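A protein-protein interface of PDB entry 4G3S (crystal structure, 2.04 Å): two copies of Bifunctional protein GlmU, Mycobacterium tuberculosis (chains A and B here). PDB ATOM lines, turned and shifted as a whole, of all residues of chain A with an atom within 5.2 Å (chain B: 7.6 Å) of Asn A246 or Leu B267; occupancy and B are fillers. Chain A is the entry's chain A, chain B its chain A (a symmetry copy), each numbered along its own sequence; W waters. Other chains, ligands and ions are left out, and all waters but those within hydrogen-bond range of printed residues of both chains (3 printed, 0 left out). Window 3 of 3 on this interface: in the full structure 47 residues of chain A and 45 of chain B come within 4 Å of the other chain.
Of the 12 printed residues of chain B, 7 touch a printed residue of chain A. Printed residues of chain B that touch a printed residue of chain A: Ala B263, Gln B266, Leu B267, Ala B268, Gly B269, Val B270 and Thr B271. Hydrophobic or aromatic side chains of chain B that line the printed part of chain A: Leu B267. Along chain B the printed residues that touch a printed residue of chain A span positions 263 to 271. Printed residues of chain A that touch a printed residue of chain B: Arg A27, Asn A246, Arg A247 and Val A248. Among the printed residues, no Asp or Glu carboxylate lies within 4 Å of a Lys or Arg side-chain nitrogen of the other chain.
The backbone carbonyl oxygen (O) of Arg A247 lies within hydrogen-bond range of the side-chain amide nitrogen (NE2) of Gln B266, at 3.4 Å. O of Gly B269 sits at hydrogen-bond distance from NH2 of Arg A247 (3.0 Å). The side-chain hydroxyl of Thr B271 sits at hydrogen-bond distance from the guanidinium group of Arg A247 (2.7 Å).
Water W2 bridges O of Arg A25 (2.7 Å) and O of Leu B267 (3.0 Å). Water W3 lies within hydrogen-bond range of N of Arg A247, O of Arg A25 and O of Gln B266. Water W1 lies within hydrogen-bond range of NE2 of Gln B266 (3.0 Å) and O of Arg A247 (3.1 Å).
Among the printed residues, merely in contact across the chains: Arg A27 with Leu B267 (3.2 Å), Arg A27 with Ala B268 (3.8 Å), Arg A27 with Gly B269 (3.5 Å), Asn A246 with Leu B267 (3.6 Å), Arg A247 with Val B270 (3.3 Å), Val A248 with Ala B263 (3.95 Å), Val A248 with Gln B266 (3.5 Å) and Val A248 with Leu B267 (3.9 Å).
No position is printed for both chains. Of the 11 pairs that touch across the chains among the printed residues, none has its exchanged pair printed and touching as well.
The side-chain sulfur (SD) of Met A26 sits close to the backbone NH (N) of Asn A246 (3.8 Å). O of Met A26 is in hydrogen-bond range of NH2 of Arg A247 (3.0 Å). The backbone carbonyl oxygen (O) of Arg A27 sits at hydrogen-bond distance from the guanidinium group (NH2) of Arg A247 (2.9 Å). The backbone NH of Val A248 is in hydrogen-bond range of the side-chain amide oxygen of Asn A246 (3.0 Å). OD1 of Asn A246 sits at hydrogen-bond distance from N of Gln A249, 2.8 Å away. N of Val B270 sits at hydrogen-bond distance from O of His B265 (2.9 Å).
Asn A246 touches just one residue of chain B: Leu B267 (3.6 Å). Leu B267 touches three residues of chain A. Of the printed residues of chain A, Ala B263 touches Val A248. Of the printed residues of chain B, Val A248 touches Ala B263, Gln B266 and Leu B267. Of the printed residues of chain A, Ala B268 touches Arg A27 (3.8 Å). Of the printed residues of chain A, Gln B266 touches Arg A247 and Val A248. Asn A245 touches none of the printed residues of chain B. Val B261 touches none of the printed residues of chain A. The nearest residue of chain B that does not touch Asn A246 is Gln B266 (5.8 Å). The nearest residue of chain A that does not touch Leu B267 is Arg A25 (4.5 Å).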
ATOM      1  N   ARG A  25       1.094  24.270  20.492  1.00  0.00           N
ATOM      2  CA  ARG A  25      -0.154  24.561  21.206  1.00  0.00           C
ATOM      3  C   ARG A  25      -1.373  24.672  20.214  1.00  0.00           C
ATOM      4  O   ARG A  25      -2.548  24.500  20.611  1.00  0.00           O
ATOM      5  CB  ARG A  25       0.065  25.797  22.047  1.00  0.00           C
ATOM      6  CG  ARG A  25       0.753  25.470  23.442  1.00  0.00           C
ATOM      7  CD  ARG A  25       1.039  26.737  24.239  1.00  0.00           C
ATOM      8  NE  ARG A  25       2.003  27.603  23.465  1.00  0.00           N
ATOM      9  CZ  ARG A  25       2.396  28.833  23.856  1.00  0.00           C
ATOM     10  NH1 ARG A  25       1.860  29.422  24.965  1.00  0.00           N
ATOM     11  NH2 ARG A  25       3.303  29.502  23.141  1.00  0.00           N
ATOM     12  N   MET A  26      -1.091  24.853  18.927  1.00  0.00           N
ATOM     13  CA  MET A  26      -2.184  24.748  17.908  1.00  0.00           C
ATOM     14  C   MET A  26      -2.691  23.291  17.736  1.00  0.00           C
ATOM     15  O   MET A  26      -3.809  23.079  17.224  1.00  0.00           O
ATOM     16  CB  MET A  26      -1.704  25.228  16.538  1.00  0.00           C
ATOM     17  CG  MET A  26      -1.223  26.705  16.518  1.00  0.00           C
ATOM     18  SD  MET A  26      -2.575  27.887  16.900  1.00  0.00           S
ATOM     19  CE  MET A  26      -3.428  27.796  15.267  1.00  0.00           C
ATOM     20  N   ARG A  27      -1.846  22.304  18.073  1.00  0.00           N
ATOM     21  CA  ARG A  27      -2.196  20.846  17.854  1.00  0.00           C
ATOM     22  C   ARG A  27      -2.612  20.604  16.433  1.00  0.00           C
ATOM     23  O   ARG A  27      -3.703  20.084  16.169  1.00  0.00           O
ATOM     24  CB  ARG A  27      -3.318  20.346  18.799  1.00  0.00           C
ATOM     25  CG  ARG A  27      -3.057  20.616  20.231  1.00  0.00           C
ATOM     26  CD  ARG A  27      -2.119  19.656  20.802  1.00  0.00           C
ATOM     27  NE  ARG A  27      -2.386  19.564  22.231  1.00  0.00           N
ATOM     28  CZ  ARG A  27      -1.674  18.834  23.083  1.00  0.00           C
ATOM     29  NH1 ARG A  27      -0.634  18.102  22.661  1.00  0.00           N
ATOM     30  NH2 ARG A  27      -2.012  18.821  24.361  1.00  0.00           N
ATOM     31  N   VAL A 244      -1.758  34.874  19.074  1.00  0.00           N
ATOM     32  CA  VAL A 244      -2.473  33.582  18.877  1.00  0.00           C
ATOM     33  C   VAL A 244      -1.528  32.414  19.060  1.00  0.00           C
ATOM     34  O   VAL A 244      -0.693  32.217  18.198  1.00  0.00           O
ATOM     35  CB  VAL A 244      -3.030  33.494  17.455  1.00  0.00           C
ATOM     36  CG1 VAL A 244      -3.663  32.159  17.131  1.00  0.00           C
ATOM     37  CG2 VAL A 244      -4.074  34.705  17.185  1.00  0.00           C
ATOM     38  N   ASN A 245      -1.647  31.694  20.170  1.00  0.00           N
ATOM     39  CA  ASN A 245      -0.852  30.503  20.442  1.00  0.00           C
ATOM     40  C   ASN A 245      -1.640  29.240  20.344  1.00  0.00           C
ATOM     41  O   ASN A 245      -1.065  28.127  20.371  1.00  0.00           O
ATOM     42  CB  ASN A 245      -0.199  30.606  21.877  1.00  0.00           C
ATOM     43  CG  ASN A 245       0.927  31.639  21.886  1.00  0.00           C
ATOM     44  OD1 ASN A 245       1.460  31.903  20.798  1.00  0.00           O
ATOM     45  ND2 ASN A 245       1.255  32.275  23.066  1.00  0.00           N
ATOM     46  N   ASN A 246      -2.980  29.368  20.338  1.00  0.00           N
ATOM     47  CA  ASN A 246      -3.811  28.147  20.247  1.00  0.00           C
ATOM     48  C   ASN A 246      -5.118  28.541  19.471  1.00  0.00           C
ATOM     49  O   ASN A 246      -5.319  29.734  19.114  1.00  0.00           O
ATOM     50  CB  ASN A 246      -4.096  27.560  21.637  1.00  0.00           C
ATOM     51  CG  ASN A 246      -4.889  28.559  22.517  1.00  0.00           C
ATOM     52  OD1 ASN A 246      -5.829  29.190  22.012  1.00  0.00           O
ATOM     53  ND2 ASN A 246      -4.497  28.720  23.794  1.00  0.00           N
ATOM     54  N   ARG A 247      -5.917  27.538  19.153  1.00  0.00           N
ATOM     55  CA  ARG A 247      -7.123  27.718  18.361  1.00  0.00           C
ATOM     56  C   ARG A 247      -8.233  28.527  19.085  1.00  0.00           C
ATOM     57  O   ARG A 247      -9.076  29.070  18.411  1.00  0.00           O
ATOM     58  CB  ARG A 247      -7.649  26.328  18.025  1.00  0.00           C
ATOM     59  CG  ARG A 247      -6.816  25.757  16.857  1.00  0.00           C
ATOM     60  CD  ARG A 247      -7.425  24.569  16.201  1.00  0.00           C
ATOM     61  NE  ARG A 247      -6.479  23.599  15.900  1.00  0.00           N
ATOM     62  CZ  ARG A 247      -6.256  22.961  14.770  1.00  0.00           C
ATOM     63  NH1 ARG A 247      -6.943  23.105  13.646  1.00  0.00           N
ATOM     64  NH2 ARG A 247      -5.330  22.036  14.877  1.00  0.00           N
ATOM     65  N   VAL A 248      -8.271  28.490  20.414  1.00  0.00           N
ATOM     66  CA  VAL A 248      -9.206  29.351  21.191  1.00  0.00           C
ATOM     67  C   VAL A 248      -8.893  30.832  20.921  1.00  0.00           C
ATOM     68  O   VAL A 248      -9.798  31.627  20.600  1.00  0.00           O
ATOM     69  CB  VAL A 248      -9.089  29.138  22.754  1.00  0.00           C
ATOM     70  CG1 VAL A 248      -9.909  30.210  23.503  1.00  0.00           C
ATOM     71  CG2 VAL A 248      -9.458  27.729  23.107  1.00  0.00           C
ATOM     72  N   GLN A 249      -7.607  31.199  21.052  1.00  0.00           N
ATOM     73  CA  GLN A 249      -7.197  32.547  20.763  1.00  0.00           C
ATOM     74  C   GLN A 249      -7.346  32.914  19.270  1.00  0.00           C
ATOM     75  O   GLN A 249      -7.636  34.055  18.931  1.00  0.00           O
ATOM     76  CB  GLN A 249      -5.750  32.789  21.216  1.00  0.00           C
ATOM     77  CG  GLN A 249      -5.623  32.733  22.760  1.00  0.00           C
ATOM     78  CD  GLN A 249      -4.229  33.125  23.194  1.00  0.00           C
ATOM     79  OE1 GLN A 249      -3.267  32.901  22.484  1.00  0.00           O
ATOM     80  NE2 GLN A 249      -4.128  33.694  24.379  1.00  0.00           N
ATOM     81  N   LEU A 250      -7.090  31.967  18.396  1.00  0.00           N
ATOM     82  CA  LEU A 250      -7.306  32.205  16.945  1.00  0.00           C
ATOM     83  C   LEU A 250      -8.803  32.647  16.701  1.00  0.00           C
ATOM     84  O   LEU A 250      -9.060  33.714  16.040  1.00  0.00           O
ATOM     85  CB  LEU A 250      -6.984  30.934  16.116  1.00  0.00           C
ATOM     86  CG  LEU A 250      -7.241  31.002  14.566  1.00  0.00           C
ATOM     87  CD1 LEU A 250      -6.547  32.215  13.942  1.00  0.00           C
ATOM     88  CD2 LEU A 250      -6.788  29.694  13.837  1.00  0.00           C
ATOM     89  N   ARG B 260     -17.295  26.182  26.863  1.00  0.00           N
ATOM     90  CA  ARG B 260     -16.320  25.303  27.460  1.00  0.00           C
ATOM     91  C   ARG B 260     -16.061  24.028  26.712  1.00  0.00           C
ATOM     92  O   ARG B 260     -14.907  23.588  26.646  1.00  0.00           O
ATOM     93  CB  ARG B 260     -16.777  24.940  28.885  1.00  0.00           C
ATOM     94  CG  ARG B 260     -16.589  26.244  29.741  1.00  0.00           C
ATOM     95  CD  ARG B 260     -17.089  26.011  31.185  1.00  0.00           C
ATOM     96  NE  ARG B 260     -17.080  27.326  31.879  1.00  0.00           N
ATOM     97  CZ  ARG B 260     -16.695  27.518  33.145  1.00  0.00           C
ATOM     98  NH1 ARG B 260     -16.352  26.496  33.961  1.00  0.00           N
ATOM     99  NH2 ARG B 260     -16.679  28.749  33.608  1.00  0.00           N
ATOM    100  N   VAL B 261     -17.132  23.381  26.241  1.00  0.00           N
ATOM    101  CA  VAL B 261     -16.968  22.192  25.402  1.00  0.00           C
ATOM    102  C   VAL B 261     -16.223  22.521  24.123  1.00  0.00           C
ATOM    103  O   VAL B 261     -15.280  21.816  23.694  1.00  0.00           O
ATOM    104  CB  VAL B 261     -18.341  21.581  25.048  1.00  0.00           C
ATOM    105  CG1 VAL B 261     -18.222  20.393  23.962  1.00  0.00           C
ATOM    106  CG2 VAL B 261     -19.024  21.028  26.408  1.00  0.00           C
ATOM    107  N   VAL B 262     -16.646  23.567  23.457  1.00  0.00           N
ATOM    108  CA  VAL B 262     -15.953  23.939  22.219  1.00  0.00           C
ATOM    109  C   VAL B 262     -14.450  24.226  22.478  1.00  0.00           C
ATOM    110  O   VAL B 262     -13.585  23.824  21.645  1.00  0.00           O
ATOM    111  CB  VAL B 262     -16.583  25.189  21.574  1.00  0.00           C
ATOM    112  CG1 VAL B 262     -15.694  25.750  20.422  1.00  0.00           C
ATOM    113  CG2 VAL B 262     -18.016  24.892  21.039  1.00  0.00           C
ATOM    114  N   ALA B 263     -14.167  24.992  23.558  1.00  0.00           N
ATOM    115  CA  ALA B 263     -12.780  25.327  23.917  1.00  0.00           C
ATOM    116  C   ALA B 263     -11.955  24.072  24.122  1.00  0.00           C
ATOM    117  O   ALA B 263     -10.780  24.046  23.658  1.00  0.00           O
ATOM    118  CB  ALA B 263     -12.633  26.284  25.196  1.00  0.00           C
ATOM    119  N   ALA B 264     -12.529  23.060  24.795  1.00  0.00           N
ATOM    120  CA  ALA B 264     -11.817  21.797  24.988  1.00  0.00           C
ATOM    121  C   ALA B 264     -11.425  21.177  23.635  1.00  0.00           C
ATOM    122  O   ALA B 264     -10.282  20.731  23.413  1.00  0.00           O
ATOM    123  CB  ALA B 264     -12.697  20.807  25.780  1.00  0.00           C
ATOM    124  N   HIS B 265     -12.367  21.180  22.697  1.00  0.00           N
ATOM    125  CA  HIS B 265     -12.050  20.735  21.359  1.00  0.00           C
ATOM    126  C   HIS B 265     -11.016  21.539  20.615  1.00  0.00           C
ATOM    127  O   HIS B 265     -10.109  20.908  19.954  1.00  0.00           O
ATOM    128  CB  HIS B 265     -13.300  20.581  20.494  1.00  0.00           C
ATOM    129  CG  HIS B 265     -14.205  19.472  20.950  1.00  0.00           C
ATOM    130  ND1 HIS B 265     -13.876  18.138  20.823  1.00  0.00           N
ATOM    131  CD2 HIS B 265     -15.443  19.509  21.518  1.00  0.00           C
ATOM    132  CE1 HIS B 265     -14.881  17.390  21.264  1.00  0.00           C
ATOM    133  NE2 HIS B 265     -15.848  18.205  21.683  1.00  0.00           N
ATOM    134  N   GLN B 266     -11.098  22.877  20.683  1.00  0.00           N
ATOM    135  CA  GLN B 266     -10.116  23.728  20.035  1.00  0.00           C
ATOM    136  C   GLN B 266      -8.685  23.481  20.605  1.00  0.00           C
ATOM    137  O   GLN B 266      -7.724  23.335  19.834  1.00  0.00           O
ATOM    138  CB  GLN B 266     -10.468  25.208  20.268  1.00  0.00           C
ATOM    139  CG  GLN B 266     -11.858  25.617  19.591  1.00  0.00           C
ATOM    140  CD  GLN B 266     -12.183  27.050  20.045  1.00  0.00           C
ATOM    141  OE1 GLN B 266     -12.342  27.303  21.227  1.00  0.00           O
ATOM    142  NE2 GLN B 266     -12.255  27.979  19.090  1.00  0.00           N
ATOM    143  N   LEU B 267      -8.572  23.385  21.932  1.00  0.00           N
ATOM    144  CA  LEU B 267      -7.253  23.073  22.590  1.00  0.00           C
ATOM    145  C   LEU B 267      -6.698  21.661  22.229  1.00  0.00           C
ATOM    146  O   LEU B 267      -5.490  21.465  22.196  1.00  0.00           O
ATOM    147  CB  LEU B 267      -7.299  23.243  24.133  1.00  0.00           C
ATOM    148  CG  LEU B 267      -7.439  24.704  24.595  1.00  0.00           C
ATOM    149  CD1 LEU B 267      -7.519  24.875  26.118  1.00  0.00           C
ATOM    150  CD2 LEU B 267      -6.293  25.579  24.075  1.00  0.00           C
ATOM    151  N   ALA B 268      -7.582  20.726  21.894  1.00  0.00           N
ATOM    152  CA  ALA B 268      -7.171  19.418  21.467  1.00  0.00           C
ATOM    153  C   ALA B 268      -6.909  19.342  19.963  1.00  0.00           C
ATOM    154  O   ALA B 268      -6.483  18.319  19.463  1.00  0.00           O
ATOM    155  CB  ALA B 268      -8.200  18.293  21.943  1.00  0.00           C
ATOM    156  N   GLY B 269      -7.156  20.402  19.208  1.00  0.00           N
ATOM    157  CA  GLY B 269      -6.769  20.334  17.794  1.00  0.00           C
ATOM    158  C   GLY B 269      -7.885  20.494  16.763  1.00  0.00           C
ATOM    159  O   GLY B 269      -7.633  20.274  15.561  1.00  0.00           O
ATOM    160  N   VAL B 270      -9.067  20.978  17.208  1.00  0.00           N
ATOM    161  CA  VAL B 270     -10.209  21.179  16.289  1.00  0.00           C
ATOM    162  C   VAL B 270     -10.340  22.690  15.986  1.00  0.00           C
ATOM    163  O   VAL B 270     -10.424  23.517  16.899  1.00  0.00           O
ATOM    164  CB  VAL B 270     -11.509  20.653  16.914  1.00  0.00           C
ATOM    165  CG1 VAL B 270     -12.710  20.932  15.996  1.00  0.00           C
ATOM    166  CG2 VAL B 270     -11.328  19.160  17.217  1.00  0.00           C
ATOM    167  N   THR B 271     -10.348  23.044  14.714  1.00  0.00           N
ATOM    168  CA  THR B 271     -10.708  24.379  14.388  1.00  0.00           C
ATOM    169  C   THR B 271     -12.208  24.604  14.482  1.00  0.00           C
ATOM    170  O   THR B 271     -13.000  23.958  13.761  1.00  0.00           O
ATOM    171  CB  THR B 271     -10.195  24.805  12.939  1.00  0.00           C
ATOM    172  OG1 THR B 271      -8.773  24.910  12.994  1.00  0.00           O
ATOM    173  CG2 THR B 271     -10.699  26.217  12.621  1.00  0.00           C
HETATM  174  O   HOH W   1     -10.861  27.492  16.472  1.00  0.00           O
HETATM  175  O   HOH W   2      -3.304  23.372  22.927  1.00  0.00           O
HETATM  176  O   HOH W   3      -5.305  24.915  19.996  1.00  0.00           O
